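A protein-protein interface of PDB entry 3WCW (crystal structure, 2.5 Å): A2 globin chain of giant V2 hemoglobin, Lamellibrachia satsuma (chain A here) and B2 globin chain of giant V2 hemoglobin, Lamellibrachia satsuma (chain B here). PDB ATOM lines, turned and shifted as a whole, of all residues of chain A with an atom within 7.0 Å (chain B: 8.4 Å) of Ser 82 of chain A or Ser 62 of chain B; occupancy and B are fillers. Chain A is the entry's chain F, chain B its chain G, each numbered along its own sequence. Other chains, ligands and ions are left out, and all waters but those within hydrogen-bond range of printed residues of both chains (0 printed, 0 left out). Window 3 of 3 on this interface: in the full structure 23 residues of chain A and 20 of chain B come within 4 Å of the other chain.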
ATOM      1  N   LEU A  77     -17.248  -1.733 -24.107  1.00  0.00           N
ATOM      2  CA  LEU A  77     -17.175  -3.029 -24.774  1.00  0.00           C
ATOM      3  C   LEU A  77     -18.273  -4.042 -24.449  1.00  0.00           C
ATOM      4  O   LEU A  77     -18.253  -5.144 -24.987  1.00  0.00           O
ATOM      5  CB  LEU A  77     -15.811  -3.665 -24.507  1.00  0.00           C
ATOM      6  CG  LEU A  77     -14.626  -2.866 -25.049  1.00  0.00           C
ATOM      7  CD1 LEU A  77     -13.305  -3.381 -24.460  1.00  0.00           C
ATOM      8  CD2 LEU A  77     -14.645  -2.963 -26.563  1.00  0.00           C
ATOM      9  N   ASP A  79     -20.971  -4.539 -25.603  1.00  0.00           N
ATOM     10  CA  ASP A  79     -21.614  -5.059 -26.806  1.00  0.00           C
ATOM     11  C   ASP A  79     -20.624  -5.822 -27.682  1.00  0.00           C
ATOM     12  O   ASP A  79     -20.957  -6.221 -28.793  1.00  0.00           O
ATOM     13  CB  ASP A  79     -22.245  -3.919 -27.621  1.00  0.00           C
ATOM     14  CG  ASP A  79     -21.214  -2.942 -28.159  1.00  0.00           C
ATOM     15  OD1 ASP A  79     -21.568  -2.134 -29.043  1.00  0.00           O
ATOM     16  OD2 ASP A  79     -20.051  -2.974 -27.699  1.00  0.00           O
ATOM     17  N   ASP A  80     -19.412  -6.019 -27.179  1.00  0.00           N
ATOM     18  CA  ASP A  80     -18.377  -6.720 -27.930  1.00  0.00           C
ATOM     19  C   ASP A  80     -17.777  -7.844 -27.077  1.00  0.00           C
ATOM     20  O   ASP A  80     -16.693  -7.697 -26.517  1.00  0.00           O
ATOM     21  CB  ASP A  80     -17.277  -5.738 -28.324  1.00  0.00           C
ATOM     22  CG  ASP A  80     -16.611  -6.106 -29.625  1.00  0.00           C
ATOM     23  OD1 ASP A  80     -16.448  -7.319 -29.876  1.00  0.00           O
ATOM     24  OD2 ASP A  80     -16.245  -5.181 -30.388  1.00  0.00           O
ATOM     25  N   GLU A  81     -18.495  -8.961 -26.986  1.00  0.00           N
ATOM     26  CA  GLU A  81     -18.065 -10.114 -26.195  1.00  0.00           C
ATOM     27  C   GLU A  81     -16.558 -10.396 -26.280  1.00  0.00           C
ATOM     28  O   GLU A  81     -15.816 -10.271 -25.298  1.00  0.00           O
ATOM     29  CB  GLU A  81     -18.833 -11.357 -26.653  1.00  0.00           C
ATOM     30  CG  GLU A  81     -18.726 -12.519 -25.694  1.00  0.00           C
ATOM     31  CD  GLU A  81     -19.437 -12.235 -24.389  1.00  0.00           C
ATOM     32  OE1 GLU A  81     -19.198 -12.975 -23.408  1.00  0.00           O
ATOM     33  OE2 GLU A  81     -20.243 -11.274 -24.351  1.00  0.00           O
ATOM     34  N   SER A  82     -16.126 -10.787 -27.473  1.00  0.00           N
ATOM     35  CA  SER A  82     -14.733 -11.106 -27.744  1.00  0.00           C
ATOM     36  C   SER A  82     -13.737 -10.102 -27.174  1.00  0.00           C
ATOM     37  O   SER A  82     -12.923 -10.445 -26.309  1.00  0.00           O
ATOM     38  CB  SER A  82     -14.532 -11.221 -29.257  1.00  0.00           C
ATOM     39  OG  SER A  82     -13.166 -11.400 -29.583  1.00  0.00           O
ATOM     40  N   VAL A  83     -13.801  -8.867 -27.663  1.00  0.00           N
ATOM     41  CA  VAL A  83     -12.885  -7.815 -27.235  1.00  0.00           C
ATOM     42  C   VAL A  83     -13.121  -7.349 -25.798  1.00  0.00           C
ATOM     43  O   VAL A  83     -12.303  -6.646 -25.221  1.00  0.00           O
ATOM     44  CB  VAL A  83     -12.953  -6.617 -28.197  1.00  0.00           C
ATOM     45  CG1 VAL A  83     -11.819  -5.648 -27.908  1.00  0.00           C
ATOM     46  CG2 VAL A  83     -12.879  -7.107 -29.633  1.00  0.00           C
ATOM     47  N   LEU A  84     -14.238  -7.756 -25.214  1.00  0.00           N
ATOM     48  CA  LEU A  84     -14.536  -7.395 -23.836  1.00  0.00           C
ATOM     49  C   LEU A  84     -13.762  -8.328 -22.909  1.00  0.00           C
ATOM     50  O   LEU A  84     -12.984  -7.883 -22.064  1.00  0.00           O
ATOM     51  CB  LEU A  84     -16.035  -7.539 -23.558  1.00  0.00           C
ATOM     52  CG  LEU A  84     -16.435  -7.475 -22.078  1.00  0.00           C
ATOM     53  CD1 LEU A  84     -16.155  -6.090 -21.540  1.00  0.00           C
ATOM     54  CD2 LEU A  84     -17.904  -7.822 -21.914  1.00  0.00           C
ATOM     55  N   ASN A  85     -13.992  -9.629 -23.079  1.00  0.00           N
ATOM     56  CA  ASN A  85     -13.328 -10.649 -22.267  1.00  0.00           C
ATOM     57  C   ASN A  85     -11.803 -10.524 -22.326  1.00  0.00           C
ATOM     58  O   ASN A  85     -11.106 -10.803 -21.346  1.00  0.00           O
ATOM     59  CB  ASN A  85     -13.767 -12.049 -22.714  1.00  0.00           C
ATOM     60  CG  ASN A  85     -15.239 -12.321 -22.422  1.00  0.00           C
ATOM     61  OD1 ASN A  85     -15.774 -11.897 -21.383  1.00  0.00           O
ATOM     62  ND2 ASN A  85     -15.895 -13.044 -23.321  1.00  0.00           N
ATOM     63  N   THR A  86     -11.285 -10.100 -23.472  1.00  0.00           N
ATOM     64  CA  THR A  86      -9.847  -9.918 -23.608  1.00  0.00           C
ATOM     65  C   THR A  86      -9.483  -8.845 -22.590  1.00  0.00           C
ATOM     66  O   THR A  86      -8.560  -9.012 -21.786  1.00  0.00           O
ATOM     67  CB  THR A  86      -9.481  -9.431 -25.028  1.00  0.00           C
ATOM     68  OG1 THR A  86      -9.993 -10.359 -25.990  1.00  0.00           O
ATOM     69  CG2 THR A  86      -7.967  -9.300 -25.195  1.00  0.00           C
ATOM     70  N   GLN A  87     -10.249  -7.757 -22.617  1.00  0.00           N
ATOM     71  CA  GLN A  87     -10.041  -6.625 -21.721  1.00  0.00           C
ATOM     72  C   GLN A  87     -10.263  -6.998 -20.252  1.00  0.00           C
ATOM     73  O   GLN A  87      -9.544  -6.528 -19.367  1.00  0.00           O
ATOM     74  CB  GLN A  87     -10.970  -5.468 -22.118  1.00  0.00           C
ATOM     75  CG  GLN A  87     -10.760  -4.193 -21.313  1.00  0.00           C
ATOM     76  CD  GLN A  87      -9.310  -3.765 -21.298  1.00  0.00           C
ATOM     77  OE1 GLN A  87      -8.632  -3.815 -22.328  1.00  0.00           O
ATOM     78  NE2 GLN A  87      -8.822  -3.333 -20.134  1.00  0.00           N
ATOM     79  N   LEU B  30     -11.603   2.835 -31.664  1.00  0.00           N
ATOM     80  CA  LEU B  30     -10.838   1.778 -32.301  1.00  0.00           C
ATOM     81  C   LEU B  30     -10.337   2.171 -33.666  1.00  0.00           C
ATOM     82  O   LEU B  30      -9.147   2.125 -33.930  1.00  0.00           O
ATOM     83  CB  LEU B  30     -11.707   0.519 -32.403  1.00  0.00           C
ATOM     84  CG  LEU B  30     -11.080  -0.863 -32.222  1.00  0.00           C
ATOM     85  CD1 LEU B  30     -10.115  -0.876 -31.044  1.00  0.00           C
ATOM     86  CD2 LEU B  30     -12.202  -1.861 -31.995  1.00  0.00           C
ATOM     87  N   GLN B  34      -6.466   2.151 -34.559  1.00  0.00           N
ATOM     88  CA  GLN B  34      -5.924   1.294 -35.614  1.00  0.00           C
ATOM     89  C   GLN B  34      -5.285   2.130 -36.725  1.00  0.00           C
ATOM     90  O   GLN B  34      -4.250   1.752 -37.276  1.00  0.00           O
ATOM     91  CB  GLN B  34      -7.028   0.411 -36.209  1.00  0.00           C
ATOM     92  CG  GLN B  34      -7.609  -0.594 -35.223  1.00  0.00           C
ATOM     93  CD  GLN B  34      -8.693  -1.497 -35.838  1.00  0.00           C
ATOM     94  OE1 GLN B  34      -9.684  -1.013 -36.394  1.00  0.00           O
ATOM     95  NE2 GLN B  34      -8.516  -2.798 -35.730  1.00  0.00           N
ATOM     96  N   VAL B  54       0.524  -8.230 -27.816  1.00  0.00           N
ATOM     97  CA  VAL B  54      -0.813  -7.785 -28.199  1.00  0.00           C
ATOM     98  C   VAL B  54      -1.095  -7.944 -29.694  1.00  0.00           C
ATOM     99  O   VAL B  54      -1.989  -7.294 -30.238  1.00  0.00           O
ATOM    100  CB  VAL B  54      -1.040  -6.311 -27.780  1.00  0.00           C
ATOM    101  CG1 VAL B  54      -0.976  -6.192 -26.261  1.00  0.00           C
ATOM    102  CG2 VAL B  54       0.017  -5.415 -28.421  1.00  0.00           C
ATOM    103  N   HIS B  55      -0.321  -8.810 -30.346  1.00  0.00           N
ATOM    104  CA  HIS B  55      -0.478  -9.112 -31.772  1.00  0.00           C
ATOM    105  C   HIS B  55      -0.394  -7.933 -32.755  1.00  0.00           C
ATOM    106  O   HIS B  55      -1.260  -7.780 -33.618  1.00  0.00           O
ATOM    107  CB  HIS B  55      -1.803  -9.853 -31.980  1.00  0.00           C
ATOM    108  CG  HIS B  55      -1.896 -11.142 -31.222  1.00  0.00           C
ATOM    109  ND1 HIS B  55      -1.578 -11.243 -29.883  1.00  0.00           N
ATOM    110  CD2 HIS B  55      -2.313 -12.373 -31.603  1.00  0.00           C
ATOM    111  CE1 HIS B  55      -1.799 -12.480 -29.472  1.00  0.00           C
ATOM    112  NE2 HIS B  55      -2.246 -13.184 -30.496  1.00  0.00           N
ATOM    113  N   GLU B  58      -1.363  -8.477 -36.536  1.00  0.00           N
ATOM    114  CA  GLU B  58      -2.775  -8.574 -36.888  1.00  0.00           C
ATOM    115  C   GLU B  58      -3.529  -7.397 -36.264  1.00  0.00           C
ATOM    116  O   GLU B  58      -4.134  -7.519 -35.193  1.00  0.00           O
ATOM    117  CB  GLU B  58      -3.337  -9.900 -36.381  1.00  0.00           C
ATOM    118  CG  GLU B  58      -4.365 -10.535 -37.296  1.00  0.00           C
ATOM    119  CD  GLU B  58      -4.537 -12.020 -37.008  1.00  0.00           C
ATOM    120  OE1 GLU B  58      -5.243 -12.705 -37.783  1.00  0.00           O
ATOM    121  OE2 GLU B  58      -3.961 -12.504 -36.003  1.00  0.00           O
ATOM    122  N   ILE B  59      -3.472  -6.260 -36.953  1.00  0.00           N
ATOM    123  CA  ILE B  59      -4.106  -5.020 -36.518  1.00  0.00           C
ATOM    124  C   ILE B  59      -5.563  -5.196 -36.112  1.00  0.00           C
ATOM    125  O   ILE B  59      -6.052  -4.504 -35.220  1.00  0.00           O
ATOM    126  CB  ILE B  59      -4.031  -3.956 -37.635  1.00  0.00           C
ATOM    127  CG1 ILE B  59      -2.572  -3.738 -38.045  1.00  0.00           C
ATOM    128  CG2 ILE B  59      -4.637  -2.646 -37.155  1.00  0.00           C
ATOM    129  CD1 ILE B  59      -2.392  -2.852 -39.269  1.00  0.00           C
ATOM    130  N   ASP B  60      -6.249  -6.130 -36.759  1.00  0.00           N
ATOM    131  CA  ASP B  60      -7.654  -6.368 -36.471  1.00  0.00           C
ATOM    132  C   ASP B  60      -7.918  -7.521 -35.492  1.00  0.00           C
ATOM    133  O   ASP B  60      -9.064  -7.925 -35.293  1.00  0.00           O
ATOM    134  CB  ASP B  60      -8.403  -6.613 -37.779  1.00  0.00           C
ATOM    135  CG  ASP B  60      -9.699  -5.831 -37.865  1.00  0.00           C
ATOM    136  OD1 ASP B  60     -10.425  -6.013 -38.868  1.00  0.00           O
ATOM    137  OD2 ASP B  60      -9.991  -5.038 -36.941  1.00  0.00           O
ATOM    138  N   SER B  61      -6.865  -8.048 -34.877  1.00  0.00           N
ATOM    139  CA  SER B  61      -7.027  -9.141 -33.923  1.00  0.00           C
ATOM    140  C   SER B  61      -7.639  -8.634 -32.618  1.00  0.00           C
ATOM    141  O   SER B  61      -7.432  -7.488 -32.228  1.00  0.00           O
ATOM    142  CB  SER B  61      -5.679  -9.781 -33.611  1.00  0.00           C
ATOM    143  OG  SER B  61      -4.895  -8.915 -32.810  1.00  0.00           O
ATOM    144  N   SER B  62      -8.378  -9.500 -31.934  1.00  0.00           N
ATOM    145  CA  SER B  62      -9.002  -9.119 -30.682  1.00  0.00           C
ATOM    146  C   SER B  62      -7.974  -8.555 -29.705  1.00  0.00           C
ATOM    147  O   SER B  62      -8.139  -7.449 -29.186  1.00  0.00           O
ATOM    148  CB  SER B  62      -9.706 -10.321 -30.060  1.00  0.00           C
ATOM    149  OG  SER B  62     -10.262  -9.976 -28.807  1.00  0.00           O
ATOM    150  N   GLU B  63      -6.906  -9.305 -29.464  1.00  0.00           N
ATOM    151  CA  GLU B  63      -5.868  -8.857 -28.541  1.00  0.00           C
ATOM    152  C   GLU B  63      -5.349  -7.447 -28.837  1.00  0.00           C
ATOM    153  O   GLU B  63      -5.176  -6.642 -27.917  1.00  0.00           O
ATOM    154  CB  GLU B  63      -4.694  -9.840 -28.535  1.00  0.00           C
ATOM    155  CG  GLU B  63      -4.707 -10.864 -29.662  1.00  0.00           C
ATOM    156  CD  GLU B  63      -5.639 -12.023 -29.389  1.00  0.00           C
ATOM    157  OE1 GLU B  63      -5.499 -12.663 -28.323  1.00  0.00           O
ATOM    158  OE2 GLU B  63      -6.508 -12.300 -30.242  1.00  0.00           O
ATOM    159  N   PHE B  64      -5.105  -7.144 -30.110  1.00  0.00           N
ATOM    160  CA  PHE B  64      -4.593  -5.826 -30.476  1.00  0.00           C
ATOM    161  C   PHE B  64      -5.671  -4.749 -30.349  1.00  0.00           C
ATOM    162  O   PHE B  64      -5.366  -3.585 -30.062  1.00  0.00           O
ATOM    163  CB  PHE B  64      -4.014  -5.840 -31.902  1.00  0.00           C
ATOM    164  CG  PHE B  64      -3.155  -4.637 -32.224  1.00  0.00           C
ATOM    165  CD1 PHE B  64      -1.984  -4.390 -31.513  1.00  0.00           C
ATOM    166  CD2 PHE B  64      -3.535  -3.731 -33.218  1.00  0.00           C
ATOM    167  CE1 PHE B  64      -1.204  -3.260 -31.781  1.00  0.00           C
ATOM    168  CE2 PHE B  64      -2.760  -2.596 -33.495  1.00  0.00           C
ATOM    169  CZ  PHE B  64      -1.591  -2.362 -32.772  1.00  0.00           C
ATOM    170  N   LYS B  65      -6.931  -5.126 -30.560  1.00  0.00           N
ATOM    171  CA  LYS B  65      -8.023  -4.157 -30.436  1.00  0.00           C
ATOM    172  C   LYS B  65      -8.033  -3.656 -29.002  1.00  0.00           C
ATOM    173  O   LYS B  65      -8.027  -2.452 -28.764  1.00  0.00           O
ATOM    174  CB  LYS B  65      -9.380  -4.797 -30.742  1.00  0.00           C
ATOM    175  CG  LYS B  65      -9.619  -5.120 -32.197  1.00  0.00           C
ATOM    176  CD  LYS B  65     -10.976  -5.778 -32.356  1.00  0.00           C
ATOM    177  CE  LYS B  65     -11.422  -5.805 -33.801  1.00  0.00           C
ATOM    178  NZ  LYS B  65     -12.779  -6.396 -33.927  1.00  0.00           N
ATOM    179  N   ALA B  66      -8.046  -4.605 -28.063  1.00  0.00           N
ATOM    180  CA  ALA B  66      -8.051  -4.314 -26.635  1.00  0.00           C
ATOM    181  C   ALA B  66      -6.889  -3.385 -26.310  1.00  0.00           C
ATOM    182  O   ALA B  66      -6.993  -2.503 -25.451  1.00  0.00           O
ATOM    183  CB  ALA B  66      -7.934  -5.615 -25.835  1.00  0.00           C
ATOM    184  N   HIS B  67      -5.781  -3.580 -27.009  1.00  0.00           N
ATOM    185  CA  HIS B  67      -4.623  -2.736 -26.791  1.00  0.00           C
ATOM    186  C   HIS B  67      -4.926  -1.326 -27.308  1.00  0.00           C
ATOM    187  O   HIS B  67      -4.623  -0.333 -26.647  1.00  0.00           O
ATOM    188  CB  HIS B  67      -3.385  -3.293 -27.511  1.00  0.00           C
ATOM    189  CG  HIS B  67      -2.192  -2.392 -27.423  1.00  0.00           C
ATOM    190  ND1 HIS B  67      -1.519  -2.164 -26.242  1.00  0.00           N
ATOM    191  CD2 HIS B  67      -1.587  -1.621 -28.359  1.00  0.00           C
ATOM    192  CE1 HIS B  67      -0.549  -1.291 -26.452  1.00  0.00           C
ATOM    193  NE2 HIS B  67      -0.568  -0.946 -27.728  1.00  0.00           N
ATOM    194  N   CYS B  68      -5.505  -1.241 -28.500  1.00  0.00           N
ATOM    195  CA  CYS B  68      -5.842   0.057 -29.071  1.00  0.00           C
ATOM    196  C   CYS B  68      -6.735   0.833 -28.108  1.00  0.00           C
ATOM    197  O   CYS B  68      -6.564   2.031 -27.910  1.00  0.00           O
ATOM    198  CB  CYS B  68      -6.542  -0.132 -30.413  1.00  0.00           C
ATOM    199  SG  CYS B  68      -5.390  -0.462 -31.764  1.00  0.00           S
ATOM    200  N   ILE B  69      -7.680   0.121 -27.502  1.00  0.00           N
ATOM    201  CA  ILE B  69      -8.597   0.718 -26.541  1.00  0.00           C
ATOM    202  C   ILE B  69      -7.810   1.131 -25.314  1.00  0.00           C
ATOM    203  O   ILE B  69      -8.071   2.181 -24.735  1.00  0.00           O
ATOM    204  CB  ILE B  69      -9.707  -0.271 -26.164  1.00  0.00           C
ATOM    205  CG1 ILE B  69     -10.672  -0.394 -27.344  1.00  0.00           C
ATOM    206  CG2 ILE B  69     -10.410   0.167 -24.893  1.00  0.00           C
ATOM    207  CD1 ILE B  69     -11.748  -1.424 -27.137  1.00  0.00           C
ATOM    208  N   ARG B  70      -6.835   0.317 -24.922  1.00  0.00           N
ATOM    209  CA  ARG B  70      -6.014   0.673 -23.773  1.00  0.00           C
ATOM    210  C   ARG B  70      -5.249   1.967 -24.057  1.00  0.00           C
ATOM    211  O   ARG B  70      -5.240   2.887 -23.237  1.00  0.00           O
ATOM    212  CB  ARG B  70      -5.033  -0.456 -23.429  1.00  0.00           C
ATOM    213  CG  ARG B  70      -5.667  -1.582 -22.593  1.00  0.00           C
ATOM    214  CD  ARG B  70      -4.632  -2.481 -21.906  1.00  0.00           C
ATOM    215  NE  ARG B  70      -3.921  -3.382 -22.817  1.00  0.00           N
ATOM    216  CZ  ARG B  70      -4.450  -4.482 -23.346  1.00  0.00           C
ATOM    217  NH1 ARG B  70      -5.702  -4.825 -23.062  1.00  0.00           N
ATOM    218  NH2 ARG B  70      -3.727  -5.247 -24.161  1.00  0.00           N
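Among the printed residues, merely in contact across the chains: Leu 77 of chain A with Ile 69 of chain B (3.3 Å), Val 83 of chain A with Lys 65 of chain B (3.6 Å), Thr 86 of chain A with Ala 66 of chain B (3.7 Å), Val 83 of chain A with Ser 62 of chain B (3.7 Å), Gln 87 of chain A with Ala 66 of chain B (3.8 Å), Val 83 of chain A with Ala 66 of chain B (3.9 Å) and Thr 86 of chain A with Glu 63 of chain B (3.97 Å).
Ser 82 of chain A touches one residue of chain B.
Of the printed residues of chain A, Ser 62 of chain B touches Ser 82, Val 83 and Thr 86.
Printed residues of chain A within 4 Å of Lys 65 of chain B: Val 83.
Printed residues of chain A within 4 Å of Ala 66 of chain B: Val 83, Thr 86 and Gln 87.
The nearest residue of chain A that does not touch Ser 62 of chain B is Leu 84 of chain A (5.8 Å).
The nearest printed residue of chain B that does not touch Thr 86 of chain A is Arg 70 of chain B (5.2 Å).
The side-chain hydroxyl (OG1) of Thr 86 of chain A sits at hydrogen-bond distance from the backbone carbonyl oxygen (O) of Ser 82 of chain A.
Printed residues of chain A that touch a printed residue of chain B: Leu 77, Ser 82, Val 83, Thr 86 and Gln 87.
Hydrophobic or aromatic side chains of chain A within 4 Å of the printed part of chain B: Leu 77 and Val 83.
Among the printed residues, no Asp or Glu carboxylate lies within 4 Å of a Lys or Arg side-chain nitrogen of the other chain.
OE1 of Gln 87 of chain A is in hydrogen-bond range of NH1 of Arg 70 of chain B.
The side-chain hydroxyl of Thr 86 of chain A lies within hydrogen-bond range of the side-chain hydroxyl of Ser 62 of chain B (2.9 Å).
OG of Ser 82 of chain A lies within hydrogen-bond range of OG of Ser 62 of chain B (3.3 Å).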
